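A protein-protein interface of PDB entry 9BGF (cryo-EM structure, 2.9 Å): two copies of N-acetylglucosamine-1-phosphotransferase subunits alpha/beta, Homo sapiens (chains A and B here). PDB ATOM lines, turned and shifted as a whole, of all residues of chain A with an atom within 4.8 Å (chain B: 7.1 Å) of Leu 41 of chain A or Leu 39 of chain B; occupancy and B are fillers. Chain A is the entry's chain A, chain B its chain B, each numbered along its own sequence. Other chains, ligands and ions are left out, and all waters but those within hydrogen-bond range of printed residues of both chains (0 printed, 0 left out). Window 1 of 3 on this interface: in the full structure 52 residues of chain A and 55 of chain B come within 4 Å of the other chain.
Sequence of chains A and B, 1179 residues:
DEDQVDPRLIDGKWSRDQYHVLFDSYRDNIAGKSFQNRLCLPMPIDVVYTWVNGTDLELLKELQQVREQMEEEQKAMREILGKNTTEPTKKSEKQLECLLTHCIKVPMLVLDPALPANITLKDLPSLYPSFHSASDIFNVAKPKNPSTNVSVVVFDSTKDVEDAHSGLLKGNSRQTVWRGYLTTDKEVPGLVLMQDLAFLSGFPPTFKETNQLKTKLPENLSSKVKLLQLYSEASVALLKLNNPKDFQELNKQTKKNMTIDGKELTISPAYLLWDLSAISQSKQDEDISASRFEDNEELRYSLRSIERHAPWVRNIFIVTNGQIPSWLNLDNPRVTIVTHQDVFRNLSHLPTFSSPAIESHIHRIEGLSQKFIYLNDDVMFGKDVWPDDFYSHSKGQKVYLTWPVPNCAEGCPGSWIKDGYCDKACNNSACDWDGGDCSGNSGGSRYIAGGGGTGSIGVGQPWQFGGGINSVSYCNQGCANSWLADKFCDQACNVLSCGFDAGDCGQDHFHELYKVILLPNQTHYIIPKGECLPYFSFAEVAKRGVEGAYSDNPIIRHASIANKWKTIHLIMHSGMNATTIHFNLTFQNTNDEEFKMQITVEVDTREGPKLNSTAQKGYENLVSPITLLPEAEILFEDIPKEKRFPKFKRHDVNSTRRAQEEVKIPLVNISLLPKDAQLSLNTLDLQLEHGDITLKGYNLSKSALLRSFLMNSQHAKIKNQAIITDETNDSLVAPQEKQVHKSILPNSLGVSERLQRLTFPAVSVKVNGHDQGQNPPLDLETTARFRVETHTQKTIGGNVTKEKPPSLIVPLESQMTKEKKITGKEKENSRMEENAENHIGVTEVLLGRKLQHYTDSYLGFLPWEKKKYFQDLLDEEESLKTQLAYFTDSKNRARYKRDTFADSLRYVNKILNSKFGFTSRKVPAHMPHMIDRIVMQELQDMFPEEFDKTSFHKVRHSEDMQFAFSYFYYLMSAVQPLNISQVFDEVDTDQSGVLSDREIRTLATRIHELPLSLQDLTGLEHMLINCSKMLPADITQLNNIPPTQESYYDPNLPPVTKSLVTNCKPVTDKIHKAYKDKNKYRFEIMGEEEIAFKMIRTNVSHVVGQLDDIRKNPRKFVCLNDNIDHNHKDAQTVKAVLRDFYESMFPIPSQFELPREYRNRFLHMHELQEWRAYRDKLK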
ATOM      1  N   LEU A  39     -34.455  19.714  20.734  1.00  0.00           N
ATOM      2  CA  LEU A  39     -34.265  18.641  19.766  1.00  0.00           C
ATOM      3  C   LEU A  39     -32.837  18.125  19.677  1.00  0.00           C
ATOM      4  O   LEU A  39     -32.641  16.991  19.240  1.00  0.00           O
ATOM      5  CB  LEU A  39     -34.698  19.102  18.365  1.00  0.00           C
ATOM      6  CG  LEU A  39     -36.139  19.573  18.161  1.00  0.00           C
ATOM      7  CD1 LEU A  39     -36.290  20.240  16.806  1.00  0.00           C
ATOM      8  CD2 LEU A  39     -37.118  18.425  18.303  1.00  0.00           C
ATOM      9  N   CYS A  40     -31.838  18.916  20.073  1.00  0.00           N
ATOM     10  CA  CYS A  40     -30.443  18.618  19.771  1.00  0.00           C
ATOM     11  C   CYS A  40     -29.629  18.186  20.988  1.00  0.00           C
ATOM     12  O   CYS A  40     -28.404  18.355  20.992  1.00  0.00           O
ATOM     13  CB  CYS A  40     -29.785  19.823  19.107  1.00  0.00           C
ATOM     14  SG  CYS A  40     -30.212  20.060  17.379  1.00  0.00           S
ATOM     15  N   LEU A  41     -30.274  17.644  22.025  1.00  0.00           N
ATOM     16  CA  LEU A  41     -29.587  17.016  23.154  1.00  0.00           C
ATOM     17  C   LEU A  41     -28.774  18.016  23.979  1.00  0.00           C
ATOM     18  O   LEU A  41     -28.570  19.159  23.550  1.00  0.00           O
ATOM     19  CB  LEU A  41     -28.686  15.882  22.651  1.00  0.00           C
ATOM     20  CG  LEU A  41     -29.375  14.564  22.296  1.00  0.00           C
ATOM     21  CD1 LEU A  41     -28.383  13.557  21.748  1.00  0.00           C
ATOM     22  CD2 LEU A  41     -30.090  14.004  23.512  1.00  0.00           C
ATOM     23  N   PRO A  42     -28.317  17.639  25.177  1.00  0.00           N
ATOM     24  CA  PRO A  42     -27.457  18.541  25.962  1.00  0.00           C
ATOM     25  C   PRO A  42     -26.023  18.522  25.452  1.00  0.00           C
ATOM     26  O   PRO A  42     -25.379  17.473  25.405  1.00  0.00           O
ATOM     27  CB  PRO A  42     -27.555  17.973  27.385  1.00  0.00           C
ATOM     28  CG  PRO A  42     -27.937  16.550  27.198  1.00  0.00           C
ATOM     29  CD  PRO A  42     -28.822  16.521  25.993  1.00  0.00           C
ATOM     30  N   MET A  43     -25.527  19.690  25.063  1.00  0.00           N
ATOM     31  CA  MET A  43     -24.147  19.867  24.644  1.00  0.00           C
ATOM     32  C   MET A  43     -23.568  21.114  25.292  1.00  0.00           C
ATOM     33  O   MET A  43     -24.279  22.105  25.485  1.00  0.00           O
ATOM     34  CB  MET A  43     -24.042  19.980  23.117  1.00  0.00           C
ATOM     35  CG  MET A  43     -24.275  18.669  22.398  1.00  0.00           C
ATOM     36  SD  MET A  43     -23.044  17.430  22.832  1.00  0.00           S
ATOM     37  CE  MET A  43     -23.946  15.928  22.479  1.00  0.00           C
ATOM     38  N   TRP A 386     -24.173   6.999  22.767  1.00  0.00           N
ATOM     39  CA  TRP A 386     -24.580   8.333  22.368  1.00  0.00           C
ATOM     40  C   TRP A 386     -25.261   8.982  23.573  1.00  0.00           C
ATOM     41  O   TRP A 386     -25.667   8.284  24.497  1.00  0.00           O
ATOM     42  CB  TRP A 386     -25.528   8.293  21.162  1.00  0.00           C
ATOM     43  CG  TRP A 386     -24.862   7.768  19.931  1.00  0.00           C
ATOM     44  CD1 TRP A 386     -24.867   6.481  19.479  1.00  0.00           C
ATOM     45  CD2 TRP A 386     -24.070   8.514  19.005  1.00  0.00           C
ATOM     46  NE1 TRP A 386     -24.134   6.383  18.324  1.00  0.00           N
ATOM     47  CE2 TRP A 386     -23.633   7.619  18.012  1.00  0.00           C
ATOM     48  CE3 TRP A 386     -23.691   9.856  18.917  1.00  0.00           C
ATOM     49  CZ2 TRP A 386     -22.840   8.022  16.945  1.00  0.00           C
ATOM     50  CZ3 TRP A 386     -22.900  10.252  17.859  1.00  0.00           C
ATOM     51  CH2 TRP A 386     -22.483   9.339  16.888  1.00  0.00           C
ATOM     52  N   PRO A 387     -25.360  10.310  23.579  1.00  0.00           N
ATOM     53  CA  PRO A 387     -26.051  10.967  24.704  1.00  0.00           C
ATOM     54  C   PRO A 387     -27.477  10.488  24.905  1.00  0.00           C
ATOM     55  O   PRO A 387     -28.027  10.680  25.995  1.00  0.00           O
ATOM     56  CB  PRO A 387     -26.000  12.449  24.319  1.00  0.00           C
ATOM     57  CG  PRO A 387     -24.785  12.562  23.479  1.00  0.00           C
ATOM     58  CD  PRO A 387     -24.692  11.282  22.705  1.00  0.00           C
ATOM     59  N   ASP A 388     -28.089   9.865  23.892  1.00  0.00           N
ATOM     60  CA  ASP A 388     -29.399   9.249  24.069  1.00  0.00           C
ATOM     61  C   ASP A 388     -29.361   8.140  25.108  1.00  0.00           C
ATOM     62  O   ASP A 388     -30.383   7.851  25.739  1.00  0.00           O
ATOM     63  CB  ASP A 388     -29.903   8.693  22.740  1.00  0.00           C
ATOM     64  CG  ASP A 388     -29.612   9.612  21.580  1.00  0.00           C
ATOM     65  OD1 ASP A 388     -29.755  10.836  21.750  1.00  0.00           O
ATOM     66  OD2 ASP A 388     -29.231   9.113  20.501  1.00  0.00           O
ATOM     67  N   TYR A 391     -29.429  10.556  28.475  1.00  0.00           N
ATOM     68  CA  TYR A 391     -30.398  11.619  28.689  1.00  0.00           C
ATOM     69  C   TYR A 391     -31.296  11.765  27.472  1.00  0.00           C
ATOM     70  O   TYR A 391     -30.843  11.627  26.333  1.00  0.00           O
ATOM     71  CB  TYR A 391     -29.688  12.943  28.982  1.00  0.00           C
ATOM     72  CG  TYR A 391     -30.606  14.077  29.369  1.00  0.00           C
ATOM     73  CD1 TYR A 391     -31.095  14.189  30.662  1.00  0.00           C
ATOM     74  CD2 TYR A 391     -30.968  15.048  28.448  1.00  0.00           C
ATOM     75  CE1 TYR A 391     -31.926  15.226  31.022  1.00  0.00           C
ATOM     76  CE2 TYR A 391     -31.799  16.091  28.800  1.00  0.00           C
ATOM     77  CZ  TYR A 391     -32.275  16.175  30.087  1.00  0.00           C
ATOM     78  OH  TYR A 391     -33.104  17.212  30.440  1.00  0.00           O
ATOM     79  N   HIS A 393     -34.595  14.590  26.352  1.00  0.00           N
ATOM     80  CA  HIS A 393     -35.327  15.775  26.785  1.00  0.00           C
ATOM     81  C   HIS A 393     -36.732  15.418  27.256  1.00  0.00           C
ATOM     82  O   HIS A 393     -37.240  16.005  28.218  1.00  0.00           O
ATOM     83  CB  HIS A 393     -35.382  16.802  25.657  1.00  0.00           C
ATOM     84  CG  HIS A 393     -34.111  17.573  25.477  1.00  0.00           C
ATOM     85  ND1 HIS A 393     -33.711  18.560  26.352  1.00  0.00           N
ATOM     86  CD2 HIS A 393     -33.158  17.512  24.517  1.00  0.00           C
ATOM     87  CE1 HIS A 393     -32.563  19.069  25.943  1.00  0.00           C
ATOM     88  NE2 HIS A 393     -32.206  18.450  24.831  1.00  0.00           N
ATOM     89  N   TYR B  26     -20.375  21.947  17.265  1.00  0.00           N
ATOM     90  CA  TYR B  26     -20.589  20.530  16.998  1.00  0.00           C
ATOM     91  C   TYR B  26     -19.293  19.805  16.674  1.00  0.00           C
ATOM     92  O   TYR B  26     -19.170  18.610  16.961  1.00  0.00           O
ATOM     93  CB  TYR B  26     -21.599  20.355  15.868  1.00  0.00           C
ATOM     94  CG  TYR B  26     -23.018  20.436  16.361  1.00  0.00           C
ATOM     95  CD1 TYR B  26     -23.650  19.318  16.880  1.00  0.00           C
ATOM     96  CD2 TYR B  26     -23.717  21.634  16.333  1.00  0.00           C
ATOM     97  CE1 TYR B  26     -24.942  19.384  17.345  1.00  0.00           C
ATOM     98  CE2 TYR B  26     -25.013  21.709  16.797  1.00  0.00           C
ATOM     99  CZ  TYR B  26     -25.621  20.581  17.303  1.00  0.00           C
ATOM    100  OH  TYR B  26     -26.913  20.649  17.767  1.00  0.00           O
ATOM    101  N   SER B  34     -18.547  16.628  13.407  1.00  0.00           N
ATOM    102  CA  SER B  34     -19.903  17.042  13.740  1.00  0.00           C
ATOM    103  C   SER B  34     -20.826  15.836  13.644  1.00  0.00           C
ATOM    104  O   SER B  34     -20.852  15.150  12.619  1.00  0.00           O
ATOM    105  CB  SER B  34     -20.376  18.155  12.806  1.00  0.00           C
ATOM    106  OG  SER B  34     -21.719  18.511  13.080  1.00  0.00           O
ATOM    107  N   PHE B  35     -21.570  15.576  14.712  1.00  0.00           N
ATOM    108  CA  PHE B  35     -22.557  14.505  14.748  1.00  0.00           C
ATOM    109  C   PHE B  35     -23.966  15.073  14.859  1.00  0.00           C
ATOM    110  O   PHE B  35     -24.841  14.485  15.495  1.00  0.00           O
ATOM    111  CB  PHE B  35     -22.277  13.544  15.901  1.00  0.00           C
ATOM    112  CG  PHE B  35     -20.875  13.018  15.919  1.00  0.00           C
ATOM    113  CD1 PHE B  35     -19.887  13.673  16.630  1.00  0.00           C
ATOM    114  CD2 PHE B  35     -20.541  11.871  15.221  1.00  0.00           C
ATOM    115  CE1 PHE B  35     -18.598  13.195  16.645  1.00  0.00           C
ATOM    116  CE2 PHE B  35     -19.249  11.390  15.236  1.00  0.00           C
ATOM    117  CZ  PHE B  35     -18.279  12.053  15.949  1.00  0.00           C
ATOM    118  N   GLN B  36     -24.199  16.225  14.224  1.00  0.00           N
ATOM    119  CA  GLN B  36     -25.492  16.890  14.343  1.00  0.00           C
ATOM    120  C   GLN B  36     -26.614  16.017  13.796  1.00  0.00           C
ATOM    121  O   GLN B  36     -27.718  15.994  14.350  1.00  0.00           O
ATOM    122  CB  GLN B  36     -25.462  18.233  13.615  1.00  0.00           C
ATOM    123  CG  GLN B  36     -26.568  19.175  14.042  1.00  0.00           C
ATOM    124  CD  GLN B  36     -26.937  20.173  12.969  1.00  0.00           C
ATOM    125  OE1 GLN B  36     -27.128  19.812  11.809  1.00  0.00           O
ATOM    126  NE2 GLN B  36     -27.042  21.441  13.352  1.00  0.00           N
ATOM    127  N   ASN B  37     -26.350  15.291  12.709  1.00  0.00           N
ATOM    128  CA  ASN B  37     -27.345  14.382  12.155  1.00  0.00           C
ATOM    129  C   ASN B  37     -27.655  13.220  13.088  1.00  0.00           C
ATOM    130  O   ASN B  37     -28.665  12.536  12.891  1.00  0.00           O
ATOM    131  CB  ASN B  37     -26.871  13.855  10.801  1.00  0.00           C
ATOM    132  CG  ASN B  37     -25.434  13.376  10.833  1.00  0.00           C
ATOM    133  OD1 ASN B  37     -24.508  14.131  10.532  1.00  0.00           O
ATOM    134  ND2 ASN B  37     -25.240  12.115  11.196  1.00  0.00           N
ATOM    135  N   ARG B  38     -26.815  12.981  14.094  1.00  0.00           N
ATOM    136  CA  ARG B  38     -27.001  11.888  15.035  1.00  0.00           C
ATOM    137  C   ARG B  38     -27.458  12.368  16.408  1.00  0.00           C
ATOM    138  O   ARG B  38     -27.726  11.540  17.285  1.00  0.00           O
ATOM    139  CB  ARG B  38     -25.694  11.090  15.154  1.00  0.00           C
ATOM    140  CG  ARG B  38     -25.804   9.751  15.865  1.00  0.00           C
ATOM    141  CD  ARG B  38     -27.036   8.986  15.440  1.00  0.00           C
ATOM    142  NE  ARG B  38     -27.119   7.692  16.103  1.00  0.00           N
ATOM    143  CZ  ARG B  38     -27.493   7.518  17.363  1.00  0.00           C
ATOM    144  NH1 ARG B  38     -27.803   8.542  18.140  1.00  0.00           N
ATOM    145  NH2 ARG B  38     -27.556   6.285  17.857  1.00  0.00           N
ATOM    146  N   LEU B  39     -27.593  13.678  16.608  1.00  0.00           N
ATOM    147  CA  LEU B  39     -27.972  14.222  17.902  1.00  0.00           C
ATOM    148  C   LEU B  39     -29.238  15.070  17.881  1.00  0.00           C
ATOM    149  O   LEU B  39     -29.736  15.415  18.957  1.00  0.00           O
ATOM    150  CB  LEU B  39     -26.827  15.071  18.480  1.00  0.00           C
ATOM    151  CG  LEU B  39     -25.427  14.465  18.599  1.00  0.00           C
ATOM    152  CD1 LEU B  39     -24.398  15.566  18.792  1.00  0.00           C
ATOM    153  CD2 LEU B  39     -25.346  13.457  19.734  1.00  0.00           C
ATOM    154  N   CYS B  40     -29.783  15.404  16.707  1.00  0.00           N
ATOM    155  CA  CYS B  40     -30.792  16.452  16.597  1.00  0.00           C
ATOM    156  C   CYS B  40     -32.150  15.959  16.102  1.00  0.00           C
ATOM    157  O   CYS B  40     -32.994  16.785  15.739  1.00  0.00           O
ATOM    158  CB  CYS B  40     -30.289  17.563  15.678  1.00  0.00           C
ATOM    159  SG  CYS B  40     -29.084  18.684  16.405  1.00  0.00           S
ATOM    160  N   LEU B  41     -32.382  14.640  16.071  1.00  0.00           N
ATOM    161  CA  LEU B  41     -33.655  14.037  15.663  1.00  0.00           C
ATOM    162  C   LEU B  41     -33.962  14.282  14.185  1.00  0.00           C
ATOM    163  O   LEU B  41     -33.490  15.266  13.602  1.00  0.00           O
ATOM    164  CB  LEU B  41     -34.803  14.554  16.539  1.00  0.00           C
ATOM    165  CG  LEU B  41     -34.922  13.934  17.934  1.00  0.00           C
ATOM    166  CD1 LEU B  41     -36.000  14.624  18.752  1.00  0.00           C
ATOM    167  CD2 LEU B  41     -35.204  12.446  17.833  1.00  0.00           C
ATOM    168  N   HIS B 393     -32.787   8.113  17.552  1.00  0.00           N
ATOM    169  CA  HIS B 393     -31.701   7.642  16.696  1.00  0.00           C
ATOM    170  C   HIS B 393     -31.093   6.349  17.225  1.00  0.00           C
ATOM    171  O   HIS B 393     -30.713   5.470  16.445  1.00  0.00           O
ATOM    172  CB  HIS B 393     -30.626   8.718  16.564  1.00  0.00           C
ATOM    173  CG  HIS B 393     -30.884   9.709  15.473  1.00  0.00           C
ATOM    174  ND1 HIS B 393     -30.989   9.345  14.148  1.00  0.00           N
ATOM    175  CD2 HIS B 393     -31.037  11.053  15.507  1.00  0.00           C
ATOM    176  CE1 HIS B 393     -31.207  10.421  13.415  1.00  0.00           C
ATOM    177  NE2 HIS B 393     -31.240  11.470  14.214  1.00  0.00           N
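The indole nitrogen (NE1) of Trp 386 of chain A sits close to the guanidinium group (NH2) of Arg 38 of chain B, at 3.5 Å.
The side-chain hydroxyl (OH) of Tyr 26 of chain B sits close to the side-chain sulfur (SG) of Cys 40 of chain A (3.4 Å).
SG of Cys 40 of chain A is disulfide-bonded to SG of Cys 40 of chain B (2.0 Å).
The backbone carbonyl oxygen of Leu 39 of chain A lies close to the backbone carbonyl oxygen of Leu 39 of chain B (3.3 Å).
NH1 of Arg 38 of chain B lies within salt-bridge range of OD2 of Asp 388 of chain A (2.8 Å).
The side-chain sulfur (SG) of Cys 40 of chain B lies within hydrogen-bond range of the side-chain hydroxyl (OH) of Tyr 26 of chain B, at 3.2 Å.
Among the printed residues, pairs that only touch across the chains: Leu 39 of chain A with Cys 40 of chain B, Leu 39 of chain A with Leu 41 of chain B, Cys 40 of chain A with Leu 39 of chain B, Leu 41 of chain A with Leu 39 of chain B, Met 43 of chain A with Leu 39 of chain B, Trp 386 of chain A with Phe 35 of chain B and Pro 387 of chain A with Leu 39 of chain B.
Printed residues of chain B within 4 Å of Cys 40 of chain A: Tyr 26 (3.3 Å), Leu 39 (3.4 Å) and Cys 40 (2.0 Å).
Leu 41 of chain A touches just one residue of chain B: Leu 39.
Printed residues of chain B within 4 Å of Met 43 of chain A: Leu 39.
Of the printed residues of chain B, Asp 388 of chain A touches Arg 38 (2.8 Å).
Of the printed residues of chain A, Phe 35 of chain B touches Trp 386 (3.6 Å).
Of chain A, only Leu 39, Cys 40, Leu 41, Met 43 and Pro 387 come within 4 Å of Leu 39 of chain B.
Of the printed residues of chain A, Leu 41 of chain B touches Leu 39.
The nearest residue of chain A that does not touch Leu 39 of chain B is Trp 386 of chain A (4.05 Å).
The nearest printed residue of chain B that does not touch Asp 388 of chain A is His 393 of chain B (4.2 Å).
Printed residues of chain A that touch a printed residue of chain B: Leu 39, Cys 40, Leu 41, Met 43, Trp 386, Pro 387 and Asp 388.
Of the 10 printed residues of chain B, 6 touch a printed residue of chain A.
Hydrophobic or aromatic side chains of chain B within 4 Å of the printed part of chain A: Tyr 26, Phe 35, Leu 39 and Leu 41.
Among the printed residues, 12 pairs touch across the chains.
Leu 39 of chain B touches its own counterpart, Leu 39 of chain A.
Leu 39 of chain A touches Cys 40 of chain B, and with the chains exchanged Cys 40 of chain A touches Leu 39 of chain B.
Leu 39 of chain A touches Leu 41 of chain B, and with the chains exchanged Leu 41 of chain A touches Leu 39 of chain B.
Cys 40 of chain B touches its own counterpart, Cys 40 of chain A.
Positions printed for both chains: 39, 40, 41 and 393.
Of the 12 pairs that touch across the chains among the printed residues, 6 have their exchanged pair printed and touching as well.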
